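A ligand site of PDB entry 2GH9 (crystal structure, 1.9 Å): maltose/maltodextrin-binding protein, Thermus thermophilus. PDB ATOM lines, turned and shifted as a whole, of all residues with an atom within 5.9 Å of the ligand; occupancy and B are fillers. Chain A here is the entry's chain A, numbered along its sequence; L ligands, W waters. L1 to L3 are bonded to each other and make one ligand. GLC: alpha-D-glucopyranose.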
ATOM      1  N   HIS A   8     -26.778  -1.938  23.418  1.00  0.00           N
ATOM      2  CA  HIS A   8     -26.134  -0.979  22.498  1.00  0.00           C
ATOM      3  C   HIS A   8     -26.734  -1.050  21.091  1.00  0.00           C
ATOM      4  O   HIS A   8     -26.261  -0.405  20.147  1.00  0.00           O
ATOM      5  CB  HIS A   8     -24.616  -1.194  22.426  1.00  0.00           C
ATOM      6  CG  HIS A   8     -24.190  -2.599  22.112  1.00  0.00           C
ATOM      7  ND1 HIS A   8     -23.960  -3.053  20.827  1.00  0.00           N
ATOM      8  CD2 HIS A   8     -23.864  -3.637  22.927  1.00  0.00           C
ATOM      9  CE1 HIS A   8     -23.564  -4.310  20.867  1.00  0.00           C
ATOM     10  NE2 HIS A   8     -23.469  -4.683  22.133  1.00  0.00           N
ATOM     11  N   PHE A   9     -27.801  -1.837  20.962  1.00  0.00           N
ATOM     12  CA  PHE A   9     -28.448  -2.003  19.688  1.00  0.00           C
ATOM     13  C   PHE A   9     -29.229  -0.738  19.311  1.00  0.00           C
ATOM     14  O   PHE A   9     -29.774  -0.019  20.174  1.00  0.00           O
ATOM     15  CB  PHE A   9     -29.437  -3.190  19.711  1.00  0.00           C
ATOM     16  CG  PHE A   9     -28.795  -4.528  19.944  1.00  0.00           C
ATOM     17  CD1 PHE A   9     -27.421  -4.711  19.903  1.00  0.00           C
ATOM     18  CD2 PHE A   9     -29.603  -5.621  20.209  1.00  0.00           C
ATOM     19  CE1 PHE A   9     -26.871  -5.951  20.114  1.00  0.00           C
ATOM     20  CE2 PHE A   9     -29.063  -6.858  20.430  1.00  0.00           C
ATOM     21  CZ  PHE A   9     -27.692  -7.029  20.363  1.00  0.00           C
ATOM     22  N   GLY A  10     -29.301  -0.485  18.011  1.00  0.00           N
ATOM     23  CA  GLY A  10     -30.196   0.516  17.453  1.00  0.00           C
ATOM     24  C   GLY A  10     -30.879  -0.054  16.247  1.00  0.00           C
ATOM     25  O   GLY A  10     -30.662  -1.222  15.886  1.00  0.00           O
ATOM     26  N   GLU A  13     -32.137  -3.895  14.796  1.00  0.00           N
ATOM     27  CA  GLU A  13     -31.706  -4.801  15.872  1.00  0.00           C
ATOM     28  C   GLU A  13     -32.405  -4.506  17.175  1.00  0.00           C
ATOM     29  O   GLU A  13     -32.845  -5.430  17.876  1.00  0.00           O
ATOM     30  CB  GLU A  13     -30.197  -4.748  16.090  1.00  0.00           C
ATOM     31  CG  GLU A  13     -29.370  -5.411  15.002  1.00  0.00           C
ATOM     32  CD  GLU A  13     -27.884  -5.421  15.342  1.00  0.00           C
ATOM     33  OE1 GLU A  13     -27.472  -4.672  16.238  1.00  0.00           O
ATOM     34  OE2 GLU A  13     -27.118  -6.194  14.711  1.00  0.00           O
ATOM     35  N   PRO A  38     -24.846   3.696  25.154  1.00  0.00           N
ATOM     36  CA  PRO A  38     -23.800   3.618  24.125  1.00  0.00           C
ATOM     37  C   PRO A  38     -22.793   2.502  24.444  1.00  0.00           C
ATOM     38  O   PRO A  38     -22.399   2.297  25.621  1.00  0.00           O
ATOM     39  CB  PRO A  38     -23.126   4.996  24.202  1.00  0.00           C
ATOM     40  CG  PRO A  38     -24.041   5.859  25.009  1.00  0.00           C
ATOM     41  CD  PRO A  38     -24.823   4.987  25.882  1.00  0.00           C
ATOM     42  N   PHE A  39     -22.394   1.786  23.403  1.00  0.00           N
ATOM     43  CA  PHE A  39     -21.516   0.625  23.512  1.00  0.00           C
ATOM     44  C   PHE A  39     -20.300   0.898  24.373  1.00  0.00           C
ATOM     45  O   PHE A  39     -19.950   0.092  25.246  1.00  0.00           O
ATOM     46  CB  PHE A  39     -21.089   0.166  22.102  1.00  0.00           C
ATOM     47  CG  PHE A  39     -20.005  -0.871  22.089  1.00  0.00           C
ATOM     48  CD1 PHE A  39     -20.316  -2.219  22.227  1.00  0.00           C
ATOM     49  CD2 PHE A  39     -18.676  -0.509  21.960  1.00  0.00           C
ATOM     50  CE1 PHE A  39     -19.328  -3.169  22.211  1.00  0.00           C
ATOM     51  CE2 PHE A  39     -17.656  -1.466  21.968  1.00  0.00           C
ATOM     52  CZ  PHE A  39     -17.978  -2.786  22.090  1.00  0.00           C
ATOM     53  N   LYS A  43     -19.561  -1.333  29.617  1.00  0.00           N
ATOM     54  CA  LYS A  43     -18.690  -2.156  30.479  1.00  0.00           C
ATOM     55  C   LYS A  43     -18.425  -1.486  31.833  1.00  0.00           C
ATOM     56  O   LYS A  43     -18.584  -2.121  32.888  1.00  0.00           O
ATOM     57  CB  LYS A  43     -17.365  -2.513  29.768  1.00  0.00           C
ATOM     58  CG  LYS A  43     -16.429  -3.421  30.622  1.00  0.00           C
ATOM     59  CD  LYS A  43     -15.306  -4.116  29.847  1.00  0.00           C
ATOM     60  CE  LYS A  43     -14.355  -3.183  29.101  1.00  0.00           C
ATOM     61  NZ  LYS A  43     -13.773  -2.080  29.923  1.00  0.00           N
ATOM     62  N   PRO A  63     -19.553  -7.892  23.863  1.00  0.00           N
ATOM     63  CA  PRO A  63     -18.528  -8.583  23.101  1.00  0.00           C
ATOM     64  C   PRO A  63     -17.692  -9.421  24.053  1.00  0.00           C
ATOM     65  O   PRO A  63     -17.515  -9.048  25.217  1.00  0.00           O
ATOM     66  CB  PRO A  63     -17.679  -7.437  22.511  1.00  0.00           C
ATOM     67  CG  PRO A  63     -17.804  -6.364  23.531  1.00  0.00           C
ATOM     68  CD  PRO A  63     -19.203  -6.480  24.094  1.00  0.00           C
ATOM     69  N   ASP A  65     -14.560  -9.975  24.437  1.00  0.00           N
ATOM     70  CA  ASP A  65     -13.307  -9.480  25.005  1.00  0.00           C
ATOM     71  C   ASP A  65     -13.509  -8.915  26.417  1.00  0.00           C
ATOM     72  O   ASP A  65     -12.571  -8.871  27.218  1.00  0.00           O
ATOM     73  CB  ASP A  65     -12.587  -8.494  24.066  1.00  0.00           C
ATOM     74  CG  ASP A  65     -13.349  -7.236  23.840  1.00  0.00           C
ATOM     75  OD1 ASP A  65     -14.466  -7.292  23.217  1.00  0.00           O
ATOM     76  OD2 ASP A  65     -12.836  -6.181  24.279  1.00  0.00           O
ATOM     77  N   TRP A  66     -14.734  -8.515  26.745  1.00  0.00           N
ATOM     78  CA  TRP A  66     -15.086  -8.015  28.080  1.00  0.00           C
ATOM     79  C   TRP A  66     -15.182  -9.094  29.189  1.00  0.00           C
ATOM     80  O   TRP A  66     -15.259  -8.738  30.365  1.00  0.00           O
ATOM     81  CB  TRP A  66     -16.448  -7.337  28.021  1.00  0.00           C
ATOM     82  CG  TRP A  66     -16.550  -6.107  27.207  1.00  0.00           C
ATOM     83  CD1 TRP A  66     -15.561  -5.529  26.441  1.00  0.00           C
ATOM     84  CD2 TRP A  66     -17.709  -5.302  27.042  1.00  0.00           C
ATOM     85  NE1 TRP A  66     -16.054  -4.403  25.835  1.00  0.00           N
ATOM     86  CE2 TRP A  66     -17.360  -4.235  26.190  1.00  0.00           C
ATOM     87  CE3 TRP A  66     -19.015  -5.354  27.555  1.00  0.00           C
ATOM     88  CZ2 TRP A  66     -18.278  -3.242  25.812  1.00  0.00           C
ATOM     89  CZ3 TRP A  66     -19.923  -4.383  27.181  1.00  0.00           C
ATOM     90  CH2 TRP A  66     -19.558  -3.332  26.327  1.00  0.00           C
ATOM     91  N   GLU A 113     -19.225 -11.872  14.545  1.00  0.00           N
ATOM     92  CA  GLU A 113     -19.086 -10.687  13.731  1.00  0.00           C
ATOM     93  C   GLU A 113     -17.622 -10.395  13.469  1.00  0.00           C
ATOM     94  O   GLU A 113     -16.758 -10.814  14.221  1.00  0.00           O
ATOM     95  CB  GLU A 113     -19.686  -9.492  14.460  1.00  0.00           C
ATOM     96  CG  GLU A 113     -19.024  -9.211  15.817  1.00  0.00           C
ATOM     97  CD  GLU A 113     -19.778  -8.231  16.659  1.00  0.00           C
ATOM     98  OE1 GLU A 113     -20.936  -7.982  16.316  1.00  0.00           O
ATOM     99  OE2 GLU A 113     -19.222  -7.693  17.653  1.00  0.00           O
ATOM    100  N   ASN A 152     -13.524   4.054  10.392  1.00  0.00           N
ATOM    101  CA  ASN A 152     -13.114   4.562  11.702  1.00  0.00           C
ATOM    102  C   ASN A 152     -11.606   4.401  11.922  1.00  0.00           C
ATOM    103  O   ASN A 152     -11.158   3.551  12.670  1.00  0.00           O
ATOM    104  CB  ASN A 152     -13.943   3.869  12.804  1.00  0.00           C
ATOM    105  CG  ASN A 152     -13.833   4.558  14.129  1.00  0.00           C
ATOM    106  OD1 ASN A 152     -13.186   5.611  14.279  1.00  0.00           O
ATOM    107  ND2 ASN A 152     -14.494   3.976  15.147  1.00  0.00           N
ATOM    108  N   ASP A 155      -9.667   3.890  15.332  1.00  0.00           N
ATOM    109  CA  ASP A 155     -10.068   2.765  16.195  1.00  0.00           C
ATOM    110  C   ASP A 155      -9.132   1.527  16.105  1.00  0.00           C
ATOM    111  O   ASP A 155      -8.906   0.982  15.037  1.00  0.00           O
ATOM    112  CB  ASP A 155     -11.516   2.399  15.849  1.00  0.00           C
ATOM    113  CG  ASP A 155     -12.180   1.505  16.887  1.00  0.00           C
ATOM    114  OD1 ASP A 155     -11.656   0.403  17.094  1.00  0.00           O
ATOM    115  OD2 ASP A 155     -13.248   1.870  17.440  1.00  0.00           O
ATOM    116  N   PRO A 156      -8.593   1.060  17.239  1.00  0.00           N
ATOM    117  CA  PRO A 156      -7.638  -0.086  17.229  1.00  0.00           C
ATOM    118  C   PRO A 156      -8.212  -1.453  16.754  1.00  0.00           C
ATOM    119  O   PRO A 156      -7.578  -2.173  15.959  1.00  0.00           O
ATOM    120  CB  PRO A 156      -7.155  -0.163  18.683  1.00  0.00           C
ATOM    121  CG  PRO A 156      -8.146   0.564  19.481  1.00  0.00           C
ATOM    122  CD  PRO A 156      -8.846   1.560  18.603  1.00  0.00           C
ATOM    123  N   TYR A 157      -9.408  -1.776  17.230  1.00  0.00           N
ATOM    124  CA  TYR A 157     -10.201  -2.914  16.690  1.00  0.00           C
ATOM    125  C   TYR A 157     -10.358  -2.893  15.151  1.00  0.00           C
ATOM    126  O   TYR A 157     -10.101  -3.891  14.480  1.00  0.00           O
ATOM    127  CB  TYR A 157     -11.576  -2.921  17.356  1.00  0.00           C
ATOM    128  CG  TYR A 157     -12.564  -3.951  16.840  1.00  0.00           C
ATOM    129  CD1 TYR A 157     -12.634  -5.191  17.401  1.00  0.00           C
ATOM    130  CD2 TYR A 157     -13.462  -3.630  15.811  1.00  0.00           C
ATOM    131  CE1 TYR A 157     -13.554  -6.124  16.985  1.00  0.00           C
ATOM    132  CE2 TYR A 157     -14.369  -4.547  15.354  1.00  0.00           C
ATOM    133  CZ  TYR A 157     -14.423  -5.813  15.956  1.00  0.00           C
ATOM    134  OH  TYR A 157     -15.314  -6.776  15.554  1.00  0.00           O
ATOM    135  N   PHE A 158     -10.774  -1.769  14.581  1.00  0.00           N
ATOM    136  CA  PHE A 158     -10.980  -1.678  13.119  1.00  0.00           C
ATOM    137  C   PHE A 158      -9.681  -1.898  12.333  1.00  0.00           C
ATOM    138  O   PHE A 158      -9.670  -2.481  11.240  1.00  0.00           O
ATOM    139  CB  PHE A 158     -11.594  -0.320  12.759  1.00  0.00           C
ATOM    140  CG  PHE A 158     -13.072  -0.262  12.934  1.00  0.00           C
ATOM    141  CD1 PHE A 158     -13.903  -0.313  11.827  1.00  0.00           C
ATOM    142  CD2 PHE A 158     -13.633  -0.165  14.184  1.00  0.00           C
ATOM    143  CE1 PHE A 158     -15.261  -0.256  11.981  1.00  0.00           C
ATOM    144  CE2 PHE A 158     -14.992  -0.121  14.339  1.00  0.00           C
ATOM    145  CZ  PHE A 158     -15.812  -0.144  13.237  1.00  0.00           C
ATOM    146  N   TYR A 215     -16.321   6.744  13.498  1.00  0.00           N
ATOM    147  CA  TYR A 215     -17.357   5.773  13.156  1.00  0.00           C
ATOM    148  C   TYR A 215     -18.554   6.432  12.465  1.00  0.00           C
ATOM    149  O   TYR A 215     -18.986   5.976  11.417  1.00  0.00           O
ATOM    150  CB  TYR A 215     -17.838   4.997  14.392  1.00  0.00           C
ATOM    151  CG  TYR A 215     -18.742   3.887  13.947  1.00  0.00           C
ATOM    152  CD1 TYR A 215     -18.217   2.662  13.533  1.00  0.00           C
ATOM    153  CD2 TYR A 215     -20.104   4.101  13.821  1.00  0.00           C
ATOM    154  CE1 TYR A 215     -19.062   1.657  13.044  1.00  0.00           C
ATOM    155  CE2 TYR A 215     -20.933   3.124  13.343  1.00  0.00           C
ATOM    156  CZ  TYR A 215     -20.409   1.895  12.959  1.00  0.00           C
ATOM    157  OH  TYR A 215     -21.263   0.956  12.478  1.00  0.00           O
ATOM    158  N   TRP A 235     -23.031  -5.513  12.436  1.00  0.00           N
ATOM    159  CA  TRP A 235     -23.826  -4.649  13.292  1.00  0.00           C
ATOM    160  C   TRP A 235     -24.406  -3.431  12.589  1.00  0.00           C
ATOM    161  O   TRP A 235     -25.329  -2.804  13.122  1.00  0.00           O
ATOM    162  CB  TRP A 235     -23.008  -4.149  14.506  1.00  0.00           C
ATOM    163  CG  TRP A 235     -21.742  -3.495  14.112  1.00  0.00           C
ATOM    164  CD1 TRP A 235     -21.562  -2.191  13.709  1.00  0.00           C
ATOM    165  CD2 TRP A 235     -20.468  -4.122  14.033  1.00  0.00           C
ATOM    166  NE1 TRP A 235     -20.229  -1.978  13.394  1.00  0.00           N
ATOM    167  CE2 TRP A 235     -19.541  -3.155  13.579  1.00  0.00           C
ATOM    168  CE3 TRP A 235     -20.011  -5.425  14.295  1.00  0.00           C
ATOM    169  CZ2 TRP A 235     -18.191  -3.427  13.421  1.00  0.00           C
ATOM    170  CZ3 TRP A 235     -18.665  -5.689  14.142  1.00  0.00           C
ATOM    171  CH2 TRP A 235     -17.775  -4.696  13.696  1.00  0.00           C
ATOM    172  N   GLY A 267     -15.332 -11.408  16.717  1.00  0.00           N
ATOM    173  CA  GLY A 267     -15.954 -11.013  17.955  1.00  0.00           C
ATOM    174  C   GLY A 267     -17.163 -11.889  18.138  1.00  0.00           C
ATOM    175  O   GLY A 267     -17.846 -12.183  17.169  1.00  0.00           O
ATOM    176  N   GLN A 269     -20.685 -11.849  20.254  1.00  0.00           N
ATOM    177  CA  GLN A 269     -21.616 -11.150  21.119  1.00  0.00           C
ATOM    178  C   GLN A 269     -22.446 -12.179  21.886  1.00  0.00           C
ATOM    179  O   GLN A 269     -22.965 -13.120  21.296  1.00  0.00           O
ATOM    180  CB  GLN A 269     -22.532 -10.255  20.288  1.00  0.00           C
ATOM    181  CG  GLN A 269     -21.820  -9.119  19.552  1.00  0.00           C
ATOM    182  CD  GLN A 269     -21.582  -7.878  20.406  1.00  0.00           C
ATOM    183  OE1 GLN A 269     -22.306  -7.598  21.352  1.00  0.00           O
ATOM    184  NE2 GLN A 269     -20.551  -7.118  20.048  1.00  0.00           N
ATOM    185  N   ARG A 305     -25.700  -9.803  11.960  1.00  0.00           N
ATOM    186  CA  ARG A 305     -24.694 -10.541  12.728  1.00  0.00           C
ATOM    187  C   ARG A 305     -24.981 -12.047  12.619  1.00  0.00           C
ATOM    188  O   ARG A 305     -26.128 -12.459  12.453  1.00  0.00           O
ATOM    189  CB  ARG A 305     -24.678 -10.119  14.206  1.00  0.00           C
ATOM    190  CG  ARG A 305     -24.499  -8.621  14.409  1.00  0.00           C
ATOM    191  CD  ARG A 305     -24.347  -8.306  15.823  1.00  0.00           C
ATOM    192  NE  ARG A 305     -24.830  -6.970  16.166  1.00  0.00           N
ATOM    193  CZ  ARG A 305     -24.196  -6.120  16.951  1.00  0.00           C
ATOM    194  NH1 ARG A 305     -23.012  -6.415  17.482  1.00  0.00           N
ATOM    195  NH2 ARG A 305     -24.747  -4.951  17.209  1.00  0.00           N
ATOM    196  N   MET A 335     -10.719 -12.158  19.226  1.00  0.00           N
ATOM    197  CA  MET A 335     -10.211 -11.316  20.280  1.00  0.00           C
ATOM    198  C   MET A 335      -9.864 -12.167  21.524  1.00  0.00           C
ATOM    199  O   MET A 335     -10.540 -13.163  21.811  1.00  0.00           O
ATOM    200  CB  MET A 335     -11.254 -10.276  20.689  1.00  0.00           C
ATOM    201  CG  MET A 335     -11.370  -9.147  19.721  1.00  0.00           C
ATOM    202  SD  MET A 335     -12.436  -7.879  20.293  1.00  0.00           S
ATOM    203  CE  MET A 335     -14.059  -8.660  20.182  1.00  0.00           C
ATOM    204  N   TRP A 345      -6.547  -1.604  24.644  1.00  0.00           N
ATOM    205  CA  TRP A 345      -7.283  -0.792  23.676  1.00  0.00           C
ATOM    206  C   TRP A 345      -6.962   0.699  23.751  1.00  0.00           C
ATOM    207  O   TRP A 345      -6.848   1.377  22.713  1.00  0.00           O
ATOM    208  CB  TRP A 345      -8.792  -0.972  23.870  1.00  0.00           C
ATOM    209  CG  TRP A 345      -9.336  -2.373  23.704  1.00  0.00           C
ATOM    210  CD1 TRP A 345     -10.007  -3.098  24.649  1.00  0.00           C
ATOM    211  CD2 TRP A 345      -9.345  -3.187  22.506  1.00  0.00           C
ATOM    212  NE1 TRP A 345     -10.397  -4.295  24.130  1.00  0.00           N
ATOM    213  CE2 TRP A 345     -10.009  -4.380  22.826  1.00  0.00           C
ATOM    214  CE3 TRP A 345      -8.842  -3.004  21.212  1.00  0.00           C
ATOM    215  CZ2 TRP A 345     -10.182  -5.407  21.892  1.00  0.00           C
ATOM    216  CZ3 TRP A 345      -9.006  -4.023  20.296  1.00  0.00           C
ATOM    217  CH2 TRP A 345      -9.682  -5.212  20.643  1.00  0.00           C
HETATM  218  C1  GLC L   1     -22.747  -0.229  17.967  1.00  0.00           C
HETATM  219  C2  GLC L   1     -22.805  -1.708  17.587  1.00  0.00           C
HETATM  220  C3  GLC L   1     -21.551  -2.408  18.079  1.00  0.00           C
HETATM  221  C4  GLC L   1     -20.320  -1.715  17.481  1.00  0.00           C
HETATM  222  C5  GLC L   1     -20.279  -0.234  17.864  1.00  0.00           C
HETATM  223  C6  GLC L   1     -19.136   0.510  17.126  1.00  0.00           C
HETATM  224  O1  GLC L   1     -22.866  -0.122  19.385  1.00  0.00           O
HETATM  225  O2  GLC L   1     -24.002  -2.325  18.123  1.00  0.00           O
HETATM  226  O3  GLC L   1     -21.563  -3.814  17.751  1.00  0.00           O
HETATM  227  O4  GLC L   1     -19.157  -2.280  18.077  1.00  0.00           O
HETATM  228  O5  GLC L   1     -21.523   0.375  17.532  1.00  0.00           O
HETATM  229  O6  GLC L   1     -19.135   1.914  17.424  1.00  0.00           O
HETATM  230  C1  GLC L   2     -18.245  -2.912  17.159  1.00  0.00           C
HETATM  231  C2  GLC L   2     -17.933  -4.302  17.679  1.00  0.00           C
HETATM  232  C3  GLC L   2     -17.138  -4.189  18.990  1.00  0.00           C
HETATM  233  C4  GLC L   2     -15.920  -3.285  18.882  1.00  0.00           C
HETATM  234  C5  GLC L   2     -16.313  -1.954  18.273  1.00  0.00           C
HETATM  235  C6  GLC L   2     -15.073  -1.091  18.003  1.00  0.00           C
HETATM  236  O2  GLC L   2     -19.152  -5.005  17.927  1.00  0.00           O
HETATM  237  O3  GLC L   2     -16.755  -5.479  19.439  1.00  0.00           O
HETATM  238  O4  GLC L   2     -15.335  -3.095  20.190  1.00  0.00           O
HETATM  239  O5  GLC L   2     -17.039  -2.144  17.036  1.00  0.00           O
HETATM  240  O6  GLC L   2     -15.370   0.307  18.033  1.00  0.00           O
HETATM  241  C1  GLC L   3     -14.050  -3.679  20.325  1.00  0.00           C
HETATM  242  C2  GLC L   3     -14.034  -4.326  21.700  1.00  0.00           C
HETATM  243  C3  GLC L   3     -14.114  -3.264  22.787  1.00  0.00           C
HETATM  244  C4  GLC L   3     -13.012  -2.239  22.568  1.00  0.00           C
HETATM  245  C5  GLC L   3     -13.040  -1.639  21.150  1.00  0.00           C
HETATM  246  C6  GLC L   3     -11.858  -0.700  20.866  1.00  0.00           C
HETATM  247  O2  GLC L   3     -15.124  -5.255  21.821  1.00  0.00           O
HETATM  248  O3  GLC L   3     -13.974  -3.869  24.066  1.00  0.00           O
HETATM  249  O4  GLC L   3     -13.161  -1.225  23.555  1.00  0.00           O
HETATM  250  O5  GLC L   3     -12.998  -2.697  20.185  1.00  0.00           O
HETATM  251  O6  GLC L   3     -12.201   0.144  19.760  1.00  0.00           O
HETATM  252  O   HOH W   1     -13.020  -2.215  26.504  1.00  0.00           O
HETATM  253  O   HOH W   2     -24.110   2.033  20.536  1.00  0.00           O
HETATM  254  O   HOH W   3     -16.005   1.472  20.577  1.00  0.00           O
HETATM  255  O   HOH W   4     -16.542   2.360  16.583  1.00  0.00           O
HETATM  256  O   HOH W   5     -16.408  -7.586  17.712  1.00  0.00           O
HETATM  257  O   HOH W   6     -15.243   0.632  23.228  1.00  0.00           O
HETATM  258  O   HOH W   7     -18.232   2.510  19.879  1.00  0.00           O
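The backbone carbonyl oxygen of His 8 is in hydrogen-bond range of an oxygen (O1) of GLC L1. NE1 of Trp 66 sits at hydrogen-bond distance from O3 of GLC L3, 2.8 Å away. O2 of GLC L2 is in hydrogen-bond range of NE2 of Gln 269, 3.3 Å away. The side-chain carboxylate of Asp 65 lies within hydrogen-bond range of an oxygen (O2) of GLC L3. A ring nitrogen (ND1) of His 8 lies within hydrogen-bond range of an oxygen (O2) of GLC L1, at 2.8 Å. The side-chain carboxylate (OD2) of Asp 155 lies within hydrogen-bond range of an oxygen (O6) of GLC L2 (2.7 Å). O2 of GLC L2 lies within hydrogen-bond range of OE2 of Glu 113, at 2.7 Å. An oxygen (O2) of GLC L1 sits at hydrogen-bond distance from the guanidinium group of Arg 305.
OE1 of Glu 113 is in salt-bridge range of NH1 of Arg 305 (2.9 Å). The side-chain carboxylate of Asp 155 sits at hydrogen-bond distance from the backbone NH of Tyr 157 (3.1 Å). The backbone NH (N) of Phe 158 sits at hydrogen-bond distance from the side-chain carboxylate (OD1) of Asp 155, at 3.4 Å. NE2 of Gln 269 is in hydrogen-bond range of OE2 of Glu 113 (2.8 Å). The side-chain amide nitrogen (ND2) of Asn 152 sits at hydrogen-bond distance from the side-chain carboxylate (OD2) of Asp 155, 3.4 Å away. The guanidinium group of Arg 305 lies within salt-bridge range of the side-chain carboxylate of Glu 13, 2.8 Å away. OE1 of Gln 269 sits at hydrogen-bond distance from NE2 of His 8 (3.2 Å). The indole nitrogen of Trp 345 lies within hydrogen-bond range of the side-chain carboxylate of Asp 65 (3.1 Å).
CB of Phe 39 touches O1 of GLC L1 (3.3 Å). Pro 63 touches the ligand. CD of Pro 156 touches O6 of GLC L3, at 3.8 Å. CB of Tyr 157 touches O5 of GLC L3, 3.2 Å away. Phe 158 touches the ligand. CB of Trp 235 touches O3 of GLC L1, 3.6 Å away. Met 335 touches the ligand. Trp 345 touches the ligand.
Water W2 lies within hydrogen-bond range of an oxygen (O1) of GLC L1 (2.7 Å), the backbone carbonyl oxygen (O) of His 8 (3.3 Å) and the backbone NH (N) of Phe 39 (3.4 Å). Water W5 lies within hydrogen-bond range of OH of Tyr 157 (2.6 Å), O3 of GLC L2 (2.7 Å) and OE2 of Glu 113 (2.8 Å). Water W4 lies within hydrogen-bond range of an oxygen (O6) of GLC L1 (2.8 Å), the side-chain amide nitrogen (ND2) of Asn 152 (3.0 Å) and the side-chain carboxylate (OD2) of Asp 155 (3.4 Å).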
